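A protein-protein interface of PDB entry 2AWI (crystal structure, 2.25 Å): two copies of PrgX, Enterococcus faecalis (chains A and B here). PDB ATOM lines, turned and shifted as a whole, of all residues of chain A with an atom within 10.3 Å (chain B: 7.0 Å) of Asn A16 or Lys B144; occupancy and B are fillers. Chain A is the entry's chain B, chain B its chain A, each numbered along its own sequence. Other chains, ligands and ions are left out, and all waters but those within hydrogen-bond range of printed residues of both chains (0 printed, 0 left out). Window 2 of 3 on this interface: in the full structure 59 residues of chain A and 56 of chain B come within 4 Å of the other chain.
Of the 9 printed residues of chain B, 4 touch a printed residue of chain A. Printed residues of chain B that touch a printed residue of chain A: Lys B144, Arg B145, Thr B146 and Thr B147. Of the 19 printed residues of chain A, 4 touch a printed residue of chain B. Printed residues of chain A that touch a printed residue of chain B: Gln A10, Glu A14, Leu A15 and Asn A16.
Of the printed residues of chain B, Asn A16 touches Lys B144 (3.1 Å). No residue of chain A comes within 4 Å of Asp B143. Of the printed residues of chain A, Thr B146 touches Glu A14. Printed residues of chain B within 4 Å of Glu A14: Arg B145, Thr B146 and Thr B147. Of the printed residues of chain B, Gln A10 touches Thr B147 (3.7 Å). Asp A21 touches none of the printed residues of chain B. The nearest residue of chain B that does not touch Asn A16 is Arg B145 (6.5 Å). The nearest residue of chain A that does not touch Lys B144 is Glu A14 (4.5 Å). The nearest printed residue of chain A that does not touch Thr B146 is Gln A10 (6.4 Å).
No position is printed for both chains. Of the 6 pairs that touch across the chains among the printed residues, none has its exchanged pair printed and touching as well.
The side-chain amino group (NZ) of Lys B144 is in hydrogen-bond range of the side-chain amide oxygen (OD1) of Asn A16. The side-chain carboxylate of Glu A14 lies within salt-bridge range of the guanidinium group of Arg B145 (2.9 Å). The side-chain hydroxyl (OG1) of Thr B147 sits at hydrogen-bond distance from the side-chain carboxylate (OE1) of Glu A14, 3.1 Å away. The side-chain hydroxyl of Thr B146 lies within hydrogen-bond range of the side-chain carboxylate of Glu A14.
The backbone carbonyl oxygen of Thr B147 is in hydrogen-bond range of the guanidinium group of Arg B145 (2.7 Å).
Among the printed residues, merely in contact across the chains: Leu A15 with Arg B145 (3.5 Å) and Gln A10 with Thr B147 (3.7 Å).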
ATOM      1  N   LEU A   8       5.290  19.067 -24.390  1.00  0.00           N
ATOM      2  CA  LEU A   8       6.048  18.568 -25.528  1.00  0.00           C
ATOM      3  C   LEU A   8       6.724  17.256 -25.137  1.00  0.00           C
ATOM      4  O   LEU A   8       6.781  16.312 -25.928  1.00  0.00           O
ATOM      5  CB  LEU A   8       7.107  19.590 -25.949  1.00  0.00           C
ATOM      6  CG  LEU A   8       6.614  20.882 -26.610  1.00  0.00           C
ATOM      7  CD1 LEU A   8       7.787  21.837 -26.812  1.00  0.00           C
ATOM      8  CD2 LEU A   8       5.957  20.561 -27.945  1.00  0.00           C
ATOM      9  N   LYS A   9       7.226  17.207 -23.905  1.00  0.00           N
ATOM     10  CA  LYS A   9       7.901  16.023 -23.397  1.00  0.00           C
ATOM     11  C   LYS A   9       6.923  14.869 -23.297  1.00  0.00           C
ATOM     12  O   LYS A   9       7.225  13.750 -23.722  1.00  0.00           O
ATOM     13  CB  LYS A   9       8.504  16.299 -22.019  1.00  0.00           C
ATOM     14  CG  LYS A   9       9.279  15.126 -21.440  1.00  0.00           C
ATOM     15  CD  LYS A   9       9.873  15.474 -20.087  1.00  0.00           C
ATOM     16  CE  LYS A   9      10.730  14.341 -19.541  1.00  0.00           C
ATOM     17  NZ  LYS A   9      11.324  14.677 -18.213  1.00  0.00           N
ATOM     18  N   GLN A  10       5.753  15.141 -22.731  1.00  0.00           N
ATOM     19  CA  GLN A  10       4.736  14.114 -22.581  1.00  0.00           C
ATOM     20  C   GLN A  10       4.364  13.572 -23.955  1.00  0.00           C
ATOM     21  O   GLN A  10       4.363  12.363 -24.174  1.00  0.00           O
ATOM     22  CB  GLN A  10       3.487  14.683 -21.897  1.00  0.00           C
ATOM     23  CG  GLN A  10       2.374  13.652 -21.734  1.00  0.00           C
ATOM     24  CD  GLN A  10       1.065  14.064 -22.398  1.00  0.00           C
ATOM     25  OE1 GLN A  10       0.304  13.215 -22.873  1.00  0.00           O
ATOM     26  NE2 GLN A  10       0.790  15.367 -22.420  1.00  0.00           N
ATOM     27  N   ILE A  11       4.053  14.478 -24.878  1.00  0.00           N
ATOM     28  CA  ILE A  11       3.672  14.100 -26.229  1.00  0.00           C
ATOM     29  C   ILE A  11       4.791  13.364 -26.952  1.00  0.00           C
ATOM     30  O   ILE A  11       4.554  12.326 -27.571  1.00  0.00           O
ATOM     31  CB  ILE A  11       3.270  15.336 -27.054  1.00  0.00           C
ATOM     32  CG1 ILE A  11       2.024  15.981 -26.436  1.00  0.00           C
ATOM     33  CG2 ILE A  11       3.023  14.942 -28.508  1.00  0.00           C
ATOM     34  CD1 ILE A  11       1.631  17.322 -27.061  1.00  0.00           C
ATOM     35  N   ARG A  12       6.007  13.898 -26.881  1.00  0.00           N
ATOM     36  CA  ARG A  12       7.138  13.265 -27.546  1.00  0.00           C
ATOM     37  C   ARG A  12       7.298  11.808 -27.111  1.00  0.00           C
ATOM     38  O   ARG A  12       7.443  10.911 -27.946  1.00  0.00           O
ATOM     39  CB  ARG A  12       8.436  14.025 -27.260  1.00  0.00           C
ATOM     40  CG  ARG A  12       9.676  13.369 -27.866  1.00  0.00           C
ATOM     41  CD  ARG A  12      10.931  14.218 -27.687  1.00  0.00           C
ATOM     42  NE  ARG A  12      11.299  14.417 -26.285  1.00  0.00           N
ATOM     43  CZ  ARG A  12      11.679  13.441 -25.460  1.00  0.00           C
ATOM     44  NH1 ARG A  12      11.741  12.187 -25.897  1.00  0.00           N
ATOM     45  NH2 ARG A  12      11.997  13.717 -24.199  1.00  0.00           N
ATOM     46  N   GLN A  13       7.266  11.578 -25.801  1.00  0.00           N
ATOM     47  CA  GLN A  13       7.424  10.233 -25.266  1.00  0.00           C
ATOM     48  C   GLN A  13       6.216   9.368 -25.571  1.00  0.00           C
ATOM     49  O   GLN A  13       6.345   8.165 -25.791  1.00  0.00           O
ATOM     50  CB  GLN A  13       7.667  10.287 -23.756  1.00  0.00           C
ATOM     51  CG  GLN A  13       8.865  11.147 -23.392  1.00  0.00           C
ATOM     52  CD  GLN A  13       9.237  11.063 -21.930  1.00  0.00           C
ATOM     53  OE1 GLN A  13       8.382  11.171 -21.049  1.00  0.00           O
ATOM     54  NE2 GLN A  13      10.527  10.884 -21.661  1.00  0.00           N
ATOM     55  N   GLU A  14       5.040   9.982 -25.586  1.00  0.00           N
ATOM     56  CA  GLU A  14       3.815   9.254 -25.882  1.00  0.00           C
ATOM     57  C   GLU A  14       3.917   8.627 -27.272  1.00  0.00           C
ATOM     58  O   GLU A  14       3.498   7.491 -27.484  1.00  0.00           O
ATOM     59  CB  GLU A  14       2.618  10.207 -25.819  1.00  0.00           C
ATOM     60  CG  GLU A  14       1.292   9.603 -26.265  1.00  0.00           C
ATOM     61  CD  GLU A  14       0.943   8.329 -25.523  1.00  0.00           C
ATOM     62  OE1 GLU A  14       1.030   8.320 -24.276  1.00  0.00           O
ATOM     63  OE2 GLU A  14       0.574   7.339 -26.182  1.00  0.00           O
ATOM     64  N   LEU A  15       4.492   9.373 -28.208  1.00  0.00           N
ATOM     65  CA  LEU A  15       4.643   8.907 -29.582  1.00  0.00           C
ATOM     66  C   LEU A  15       5.975   8.203 -29.793  1.00  0.00           C
ATOM     67  O   LEU A  15       6.357   7.896 -30.925  1.00  0.00           O
ATOM     68  CB  LEU A  15       4.532  10.084 -30.552  1.00  0.00           C
ATOM     69  CG  LEU A  15       3.275  10.953 -30.427  1.00  0.00           C
ATOM     70  CD1 LEU A  15       3.348  12.095 -31.441  1.00  0.00           C
ATOM     71  CD2 LEU A  15       2.025  10.101 -30.653  1.00  0.00           C
ATOM     72  N   ASN A  16       6.682   7.958 -28.695  1.00  0.00           N
ATOM     73  CA  ASN A  16       7.970   7.279 -28.732  1.00  0.00           C
ATOM     74  C   ASN A  16       8.998   7.974 -29.631  1.00  0.00           C
ATOM     75  O   ASN A  16       9.634   7.336 -30.474  1.00  0.00           O
ATOM     76  CB  ASN A  16       7.780   5.828 -29.191  1.00  0.00           C
ATOM     77  CG  ASN A  16       8.889   4.911 -28.703  1.00  0.00           C
ATOM     78  OD1 ASN A  16       8.999   3.767 -29.144  1.00  0.00           O
ATOM     79  ND2 ASN A  16       9.709   5.404 -27.779  1.00  0.00           N
ATOM     80  N   TYR A  17       9.151   9.282 -29.451  1.00  0.00           N
ATOM     81  CA  TYR A  17      10.117  10.055 -30.223  1.00  0.00           C
ATOM     82  C   TYR A  17      11.309  10.359 -29.319  1.00  0.00           C
ATOM     83  O   TYR A  17      11.163  10.478 -28.100  1.00  0.00           O
ATOM     84  CB  TYR A  17       9.516  11.386 -30.696  1.00  0.00           C
ATOM     85  CG  TYR A  17       8.638  11.320 -31.926  1.00  0.00           C
ATOM     86  CD1 TYR A  17       9.132  10.845 -33.138  1.00  0.00           C
ATOM     87  CD2 TYR A  17       7.322  11.775 -31.887  1.00  0.00           C
ATOM     88  CE1 TYR A  17       8.334  10.829 -34.288  1.00  0.00           C
ATOM     89  CE2 TYR A  17       6.516  11.761 -33.024  1.00  0.00           C
ATOM     90  CZ  TYR A  17       7.028  11.289 -34.221  1.00  0.00           C
ATOM     91  OH  TYR A  17       6.233  11.274 -35.345  1.00  0.00           O
ATOM     92  N   HIS A  18      12.486  10.485 -29.916  1.00  0.00           N
ATOM     93  CA  HIS A  18      13.680  10.805 -29.149  1.00  0.00           C
ATOM     94  C   HIS A  18      13.942  12.297 -29.303  1.00  0.00           C
ATOM     95  O   HIS A  18      13.622  12.885 -30.338  1.00  0.00           O
ATOM     96  CB  HIS A  18      14.870   9.993 -29.656  1.00  0.00           C
ATOM     97  CG  HIS A  18      14.701   8.514 -29.489  1.00  0.00           C
ATOM     98  ND1 HIS A  18      14.385   7.935 -28.279  1.00  0.00           N
ATOM     99  CD2 HIS A  18      14.809   7.498 -30.376  1.00  0.00           C
ATOM    100  CE1 HIS A  18      14.306   6.624 -28.427  1.00  0.00           C
ATOM    101  NE2 HIS A  18      14.561   6.333 -29.691  1.00  0.00           N
ATOM    102  N   GLN A  19      14.514  12.907 -28.271  1.00  0.00           N
ATOM    103  CA  GLN A  19      14.792  14.335 -28.295  1.00  0.00           C
ATOM    104  C   GLN A  19      15.386  14.751 -29.631  1.00  0.00           C
ATOM    105  O   GLN A  19      15.044  15.803 -30.175  1.00  0.00           O
ATOM    106  CB  GLN A  19      15.742  14.704 -27.161  1.00  0.00           C
ATOM    107  CG  GLN A  19      15.351  14.084 -25.836  1.00  0.00           C
ATOM    108  CD  GLN A  19      16.138  14.646 -24.676  1.00  0.00           C
ATOM    109  OE1 GLN A  19      15.787  15.688 -24.122  1.00  0.00           O
ATOM    110  NE2 GLN A  19      17.217  13.965 -24.309  1.00  0.00           N
ATOM    111  N   ILE A  20      16.260  13.904 -30.162  1.00  0.00           N
ATOM    112  CA  ILE A  20      16.921  14.158 -31.436  1.00  0.00           C
ATOM    113  C   ILE A  20      15.907  14.433 -32.543  1.00  0.00           C
ATOM    114  O   ILE A  20      16.111  15.315 -33.376  1.00  0.00           O
ATOM    115  CB  ILE A  20      17.795  12.957 -31.864  1.00  0.00           C
ATOM    116  CG1 ILE A  20      18.757  12.572 -30.734  1.00  0.00           C
ATOM    117  CG2 ILE A  20      18.584  13.313 -33.116  1.00  0.00           C
ATOM    118  CD1 ILE A  20      18.091  11.915 -29.524  1.00  0.00           C
ATOM    119  N   ASP A  21      14.818  13.673 -32.550  1.00  0.00           N
ATOM    120  CA  ASP A  21      13.778  13.835 -33.558  1.00  0.00           C
ATOM    121  C   ASP A  21      13.145  15.225 -33.508  1.00  0.00           C
ATOM    122  O   ASP A  21      12.652  15.731 -34.516  1.00  0.00           O
ATOM    123  CB  ASP A  21      12.693  12.773 -33.368  1.00  0.00           C
ATOM    124  CG  ASP A  21      13.249  11.366 -33.384  1.00  0.00           C
ATOM    125  OD1 ASP A  21      13.848  10.976 -34.410  1.00  0.00           O
ATOM    126  OD2 ASP A  21      13.087  10.649 -32.372  1.00  0.00           O
ATOM    127  N   LEU A  22      13.166  15.838 -32.329  1.00  0.00           N
ATOM    128  CA  LEU A  22      12.583  17.161 -32.142  1.00  0.00           C
ATOM    129  C   LEU A  22      13.521  18.336 -32.420  1.00  0.00           C
ATOM    130  O   LEU A  22      13.188  19.218 -33.214  1.00  0.00           O
ATOM    131  CB  LEU A  22      12.015  17.283 -30.727  1.00  0.00           C
ATOM    132  CG  LEU A  22      10.571  16.811 -30.507  1.00  0.00           C
ATOM    133  CD1 LEU A  22       9.620  17.856 -31.069  1.00  0.00           C
ATOM    134  CD2 LEU A  22      10.338  15.454 -31.165  1.00  0.00           C
ATOM    135  N   GLU A  36      12.299  21.513 -22.467  1.00  0.00           N
ATOM    136  CA  GLU A  36      11.368  20.533 -21.896  1.00  0.00           C
ATOM    137  C   GLU A  36      11.207  20.616 -20.385  1.00  0.00           C
ATOM    138  O   GLU A  36      10.241  20.092 -19.828  1.00  0.00           O
ATOM    139  CB  GLU A  36      11.764  19.101 -22.270  1.00  0.00           C
ATOM    140  CG  GLU A  36      11.644  18.781 -23.746  1.00  0.00           C
ATOM    141  CD  GLU A  36      11.540  17.288 -24.014  1.00  0.00           C
ATOM    142  OE1 GLU A  36      12.257  16.511 -23.353  1.00  0.00           O
ATOM    143  OE2 GLU A  36      10.746  16.892 -24.895  1.00  0.00           O
ATOM    144  N   ARG A  53       6.571  18.253 -36.045  1.00  0.00           N
ATOM    145  CA  ARG A  53       7.341  17.030 -35.864  1.00  0.00           C
ATOM    146  C   ARG A  53       6.511  16.022 -35.083  1.00  0.00           C
ATOM    147  O   ARG A  53       6.510  14.828 -35.387  1.00  0.00           O
ATOM    148  CB  ARG A  53       8.632  17.332 -35.103  1.00  0.00           C
ATOM    149  CG  ARG A  53       9.512  18.369 -35.777  1.00  0.00           C
ATOM    150  CD  ARG A  53      10.466  17.745 -36.772  1.00  0.00           C
ATOM    151  NE  ARG A  53      11.832  17.777 -36.260  1.00  0.00           N
ATOM    152  CZ  ARG A  53      12.805  18.525 -36.770  1.00  0.00           C
ATOM    153  NH1 ARG A  53      12.569  19.307 -37.815  1.00  0.00           N
ATOM    154  NH2 ARG A  53      14.014  18.497 -36.226  1.00  0.00           N
ATOM    155  N   LEU A  54       5.802  16.519 -34.074  1.00  0.00           N
ATOM    156  CA  LEU A  54       4.964  15.681 -33.231  1.00  0.00           C
ATOM    157  C   LEU A  54       3.712  15.215 -33.968  1.00  0.00           C
ATOM    158  O   LEU A  54       3.111  14.199 -33.610  1.00  0.00           O
ATOM    159  CB  LEU A  54       4.554  16.457 -31.979  1.00  0.00           C
ATOM    160  CG  LEU A  54       5.664  16.894 -31.020  1.00  0.00           C
ATOM    161  CD1 LEU A  54       5.087  17.805 -29.953  1.00  0.00           C
ATOM    162  CD2 LEU A  54       6.305  15.672 -30.387  1.00  0.00           C
ATOM    163  N   VAL A  56       1.020  16.705 -33.894  1.00  0.00           N
ATOM    164  CA  VAL A  56      -0.114  17.142 -33.086  1.00  0.00           C
ATOM    165  C   VAL A  56      -0.327  18.619 -33.389  1.00  0.00           C
ATOM    166  O   VAL A  56       0.635  19.358 -33.590  1.00  0.00           O
ATOM    167  CB  VAL A  56       0.162  16.942 -31.580  1.00  0.00           C
ATOM    168  CG1 VAL A  56      -1.005  17.470 -30.745  1.00  0.00           C
ATOM    169  CG2 VAL A  56       0.391  15.469 -31.304  1.00  0.00           C
ATOM    170  N   LYS B 139      -0.658  -1.030 -36.352  1.00  0.00           N
ATOM    171  CA  LYS B 139      -0.029  -1.613 -35.170  1.00  0.00           C
ATOM    172  C   LYS B 139       1.175  -0.766 -34.778  1.00  0.00           C
ATOM    173  O   LYS B 139       1.375  -0.448 -33.608  1.00  0.00           O
ATOM    174  CB  LYS B 139       0.420  -3.050 -35.449  1.00  0.00           C
ATOM    175  CG  LYS B 139      -0.710  -4.066 -35.484  1.00  0.00           C
ATOM    176  CD  LYS B 139      -0.180  -5.459 -35.782  1.00  0.00           C
ATOM    177  CE  LYS B 139      -1.261  -6.521 -35.616  1.00  0.00           C
ATOM    178  NZ  LYS B 139      -2.451  -6.286 -36.481  1.00  0.00           N
ATOM    179  N   HIS B 140       1.974  -0.396 -35.770  1.00  0.00           N
ATOM    180  CA  HIS B 140       3.151   0.415 -35.523  1.00  0.00           C
ATOM    181  C   HIS B 140       2.801   1.757 -34.876  1.00  0.00           C
ATOM    182  O   HIS B 140       3.541   2.263 -34.029  1.00  0.00           O
ATOM    183  CB  HIS B 140       3.899   0.646 -36.832  1.00  0.00           C
ATOM    184  CG  HIS B 140       5.090   1.537 -36.694  1.00  0.00           C
ATOM    185  ND1 HIS B 140       4.984   2.905 -36.562  1.00  0.00           N
ATOM    186  CD2 HIS B 140       6.412   1.257 -36.653  1.00  0.00           C
ATOM    187  CE1 HIS B 140       6.190   3.429 -36.446  1.00  0.00           C
ATOM    188  NE2 HIS B 140       7.076   2.450 -36.498  1.00  0.00           N
ATOM    189  N   LEU B 141       1.665   2.325 -35.264  1.00  0.00           N
ATOM    190  CA  LEU B 141       1.240   3.605 -34.723  1.00  0.00           C
ATOM    191  C   LEU B 141       0.469   3.509 -33.412  1.00  0.00           C
ATOM    192  O   LEU B 141       0.613   4.377 -32.552  1.00  0.00           O
ATOM    193  CB  LEU B 141       0.368   4.348 -35.742  1.00  0.00           C
ATOM    194  CG  LEU B 141       1.014   4.746 -37.070  1.00  0.00           C
ATOM    195  CD1 LEU B 141      -0.070   5.184 -38.046  1.00  0.00           C
ATOM    196  CD2 LEU B 141       2.032   5.850 -36.834  1.00  0.00           C
ATOM    197  N   TYR B 142      -0.334   2.459 -33.244  1.00  0.00           N
ATOM    198  CA  TYR B 142      -1.154   2.356 -32.039  1.00  0.00           C
ATOM    199  C   TYR B 142      -0.903   1.287 -30.983  1.00  0.00           C
ATOM    200  O   TYR B 142      -1.556   1.308 -29.946  1.00  0.00           O
ATOM    201  CB  TYR B 142      -2.630   2.324 -32.450  1.00  0.00           C
ATOM    202  CG  TYR B 142      -3.075   3.631 -33.066  1.00  0.00           C
ATOM    203  CD1 TYR B 142      -3.242   4.771 -32.275  1.00  0.00           C
ATOM    204  CD2 TYR B 142      -3.244   3.758 -34.450  1.00  0.00           C
ATOM    205  CE1 TYR B 142      -3.555   6.002 -32.841  1.00  0.00           C
ATOM    206  CE2 TYR B 142      -3.559   4.985 -35.025  1.00  0.00           C
ATOM    207  CZ  TYR B 142      -3.708   6.102 -34.213  1.00  0.00           C
ATOM    208  OH  TYR B 142      -3.988   7.323 -34.770  1.00  0.00           O
ATOM    209  N   ASP B 143       0.033   0.371 -31.212  1.00  0.00           N
ATOM    210  CA  ASP B 143       0.314  -0.687 -30.236  1.00  0.00           C
ATOM    211  C   ASP B 143       0.803  -0.228 -28.855  1.00  0.00           C
ATOM    212  O   ASP B 143       0.593  -0.923 -27.863  1.00  0.00           O
ATOM    213  CB  ASP B 143       1.329  -1.682 -30.815  1.00  0.00           C
ATOM    214  CG  ASP B 143       0.665  -2.839 -31.542  1.00  0.00           C
ATOM    215  OD1 ASP B 143       1.388  -3.700 -32.090  1.00  0.00           O
ATOM    216  OD2 ASP B 143      -0.583  -2.892 -31.560  1.00  0.00           O
ATOM    217  N   LYS B 144       1.441   0.935 -28.779  1.00  0.00           N
ATOM    218  CA  LYS B 144       1.973   1.414 -27.505  1.00  0.00           C
ATOM    219  C   LYS B 144       1.264   2.618 -26.897  1.00  0.00           C
ATOM    220  O   LYS B 144       1.591   3.022 -25.786  1.00  0.00           O
ATOM    221  CB  LYS B 144       3.448   1.777 -27.664  1.00  0.00           C
ATOM    222  CG  LYS B 144       4.280   0.759 -28.410  1.00  0.00           C
ATOM    223  CD  LYS B 144       5.675   1.311 -28.671  1.00  0.00           C
ATOM    224  CE  LYS B 144       6.464   0.427 -29.626  1.00  0.00           C
ATOM    225  NZ  LYS B 144       7.807   1.002 -29.915  1.00  0.00           N
ATOM    226  N   ARG B 145       0.305   3.190 -27.618  1.00  0.00           N
ATOM    227  CA  ARG B 145      -0.413   4.378 -27.162  1.00  0.00           C
ATOM    228  C   ARG B 145      -1.199   4.271 -25.853  1.00  0.00           C
ATOM    229  O   ARG B 145      -1.686   3.198 -25.500  1.00  0.00           O
ATOM    230  CB  ARG B 145      -1.337   4.854 -28.282  1.00  0.00           C
ATOM    231  CG  ARG B 145      -0.599   5.153 -29.590  1.00  0.00           C
ATOM    232  CD  ARG B 145       0.444   6.250 -29.378  1.00  0.00           C
ATOM    233  NE  ARG B 145      -0.182   7.510 -28.981  1.00  0.00           N
ATOM    234  CZ  ARG B 145      -0.831   8.325 -29.812  1.00  0.00           C
ATOM    235  NH1 ARG B 145      -0.940   8.028 -31.107  1.00  0.00           N
ATOM    236  NH2 ARG B 145      -1.396   9.429 -29.339  1.00  0.00           N
ATOM    237  N   THR B 146      -1.309   5.396 -25.138  1.00  0.00           N
ATOM    238  CA  THR B 146      -2.053   5.465 -23.872  1.00  0.00           C
ATOM    239  C   THR B 146      -2.986   6.686 -23.858  1.00  0.00           C
ATOM    240  O   THR B 146      -4.010   6.694 -23.176  1.00  0.00           O
ATOM    241  CB  THR B 146      -1.109   5.548 -22.628  1.00  0.00           C
ATOM    242  OG1 THR B 146      -0.524   6.855 -22.538  1.00  0.00           O
ATOM    243  CG2 THR B 146       0.003   4.506 -22.724  1.00  0.00           C
ATOM    244  N   THR B 147      -2.615   7.723 -24.601  1.00  0.00           N
ATOM    245  CA  THR B 147      -3.416   8.943 -24.703  1.00  0.00           C
ATOM    246  C   THR B 147      -3.454   9.345 -26.163  1.00  0.00           C
ATOM    247  O   THR B 147      -2.461   9.209 -26.875  1.00  0.00           O
ATOM    248  CB  THR B 147      -2.825  10.119 -23.887  1.00  0.00           C
ATOM    249  OG1 THR B 147      -1.408  10.186 -24.085  1.00  0.00           O
ATOM    250  CG2 THR B 147      -3.136   9.956 -22.422  1.00  0.00           C
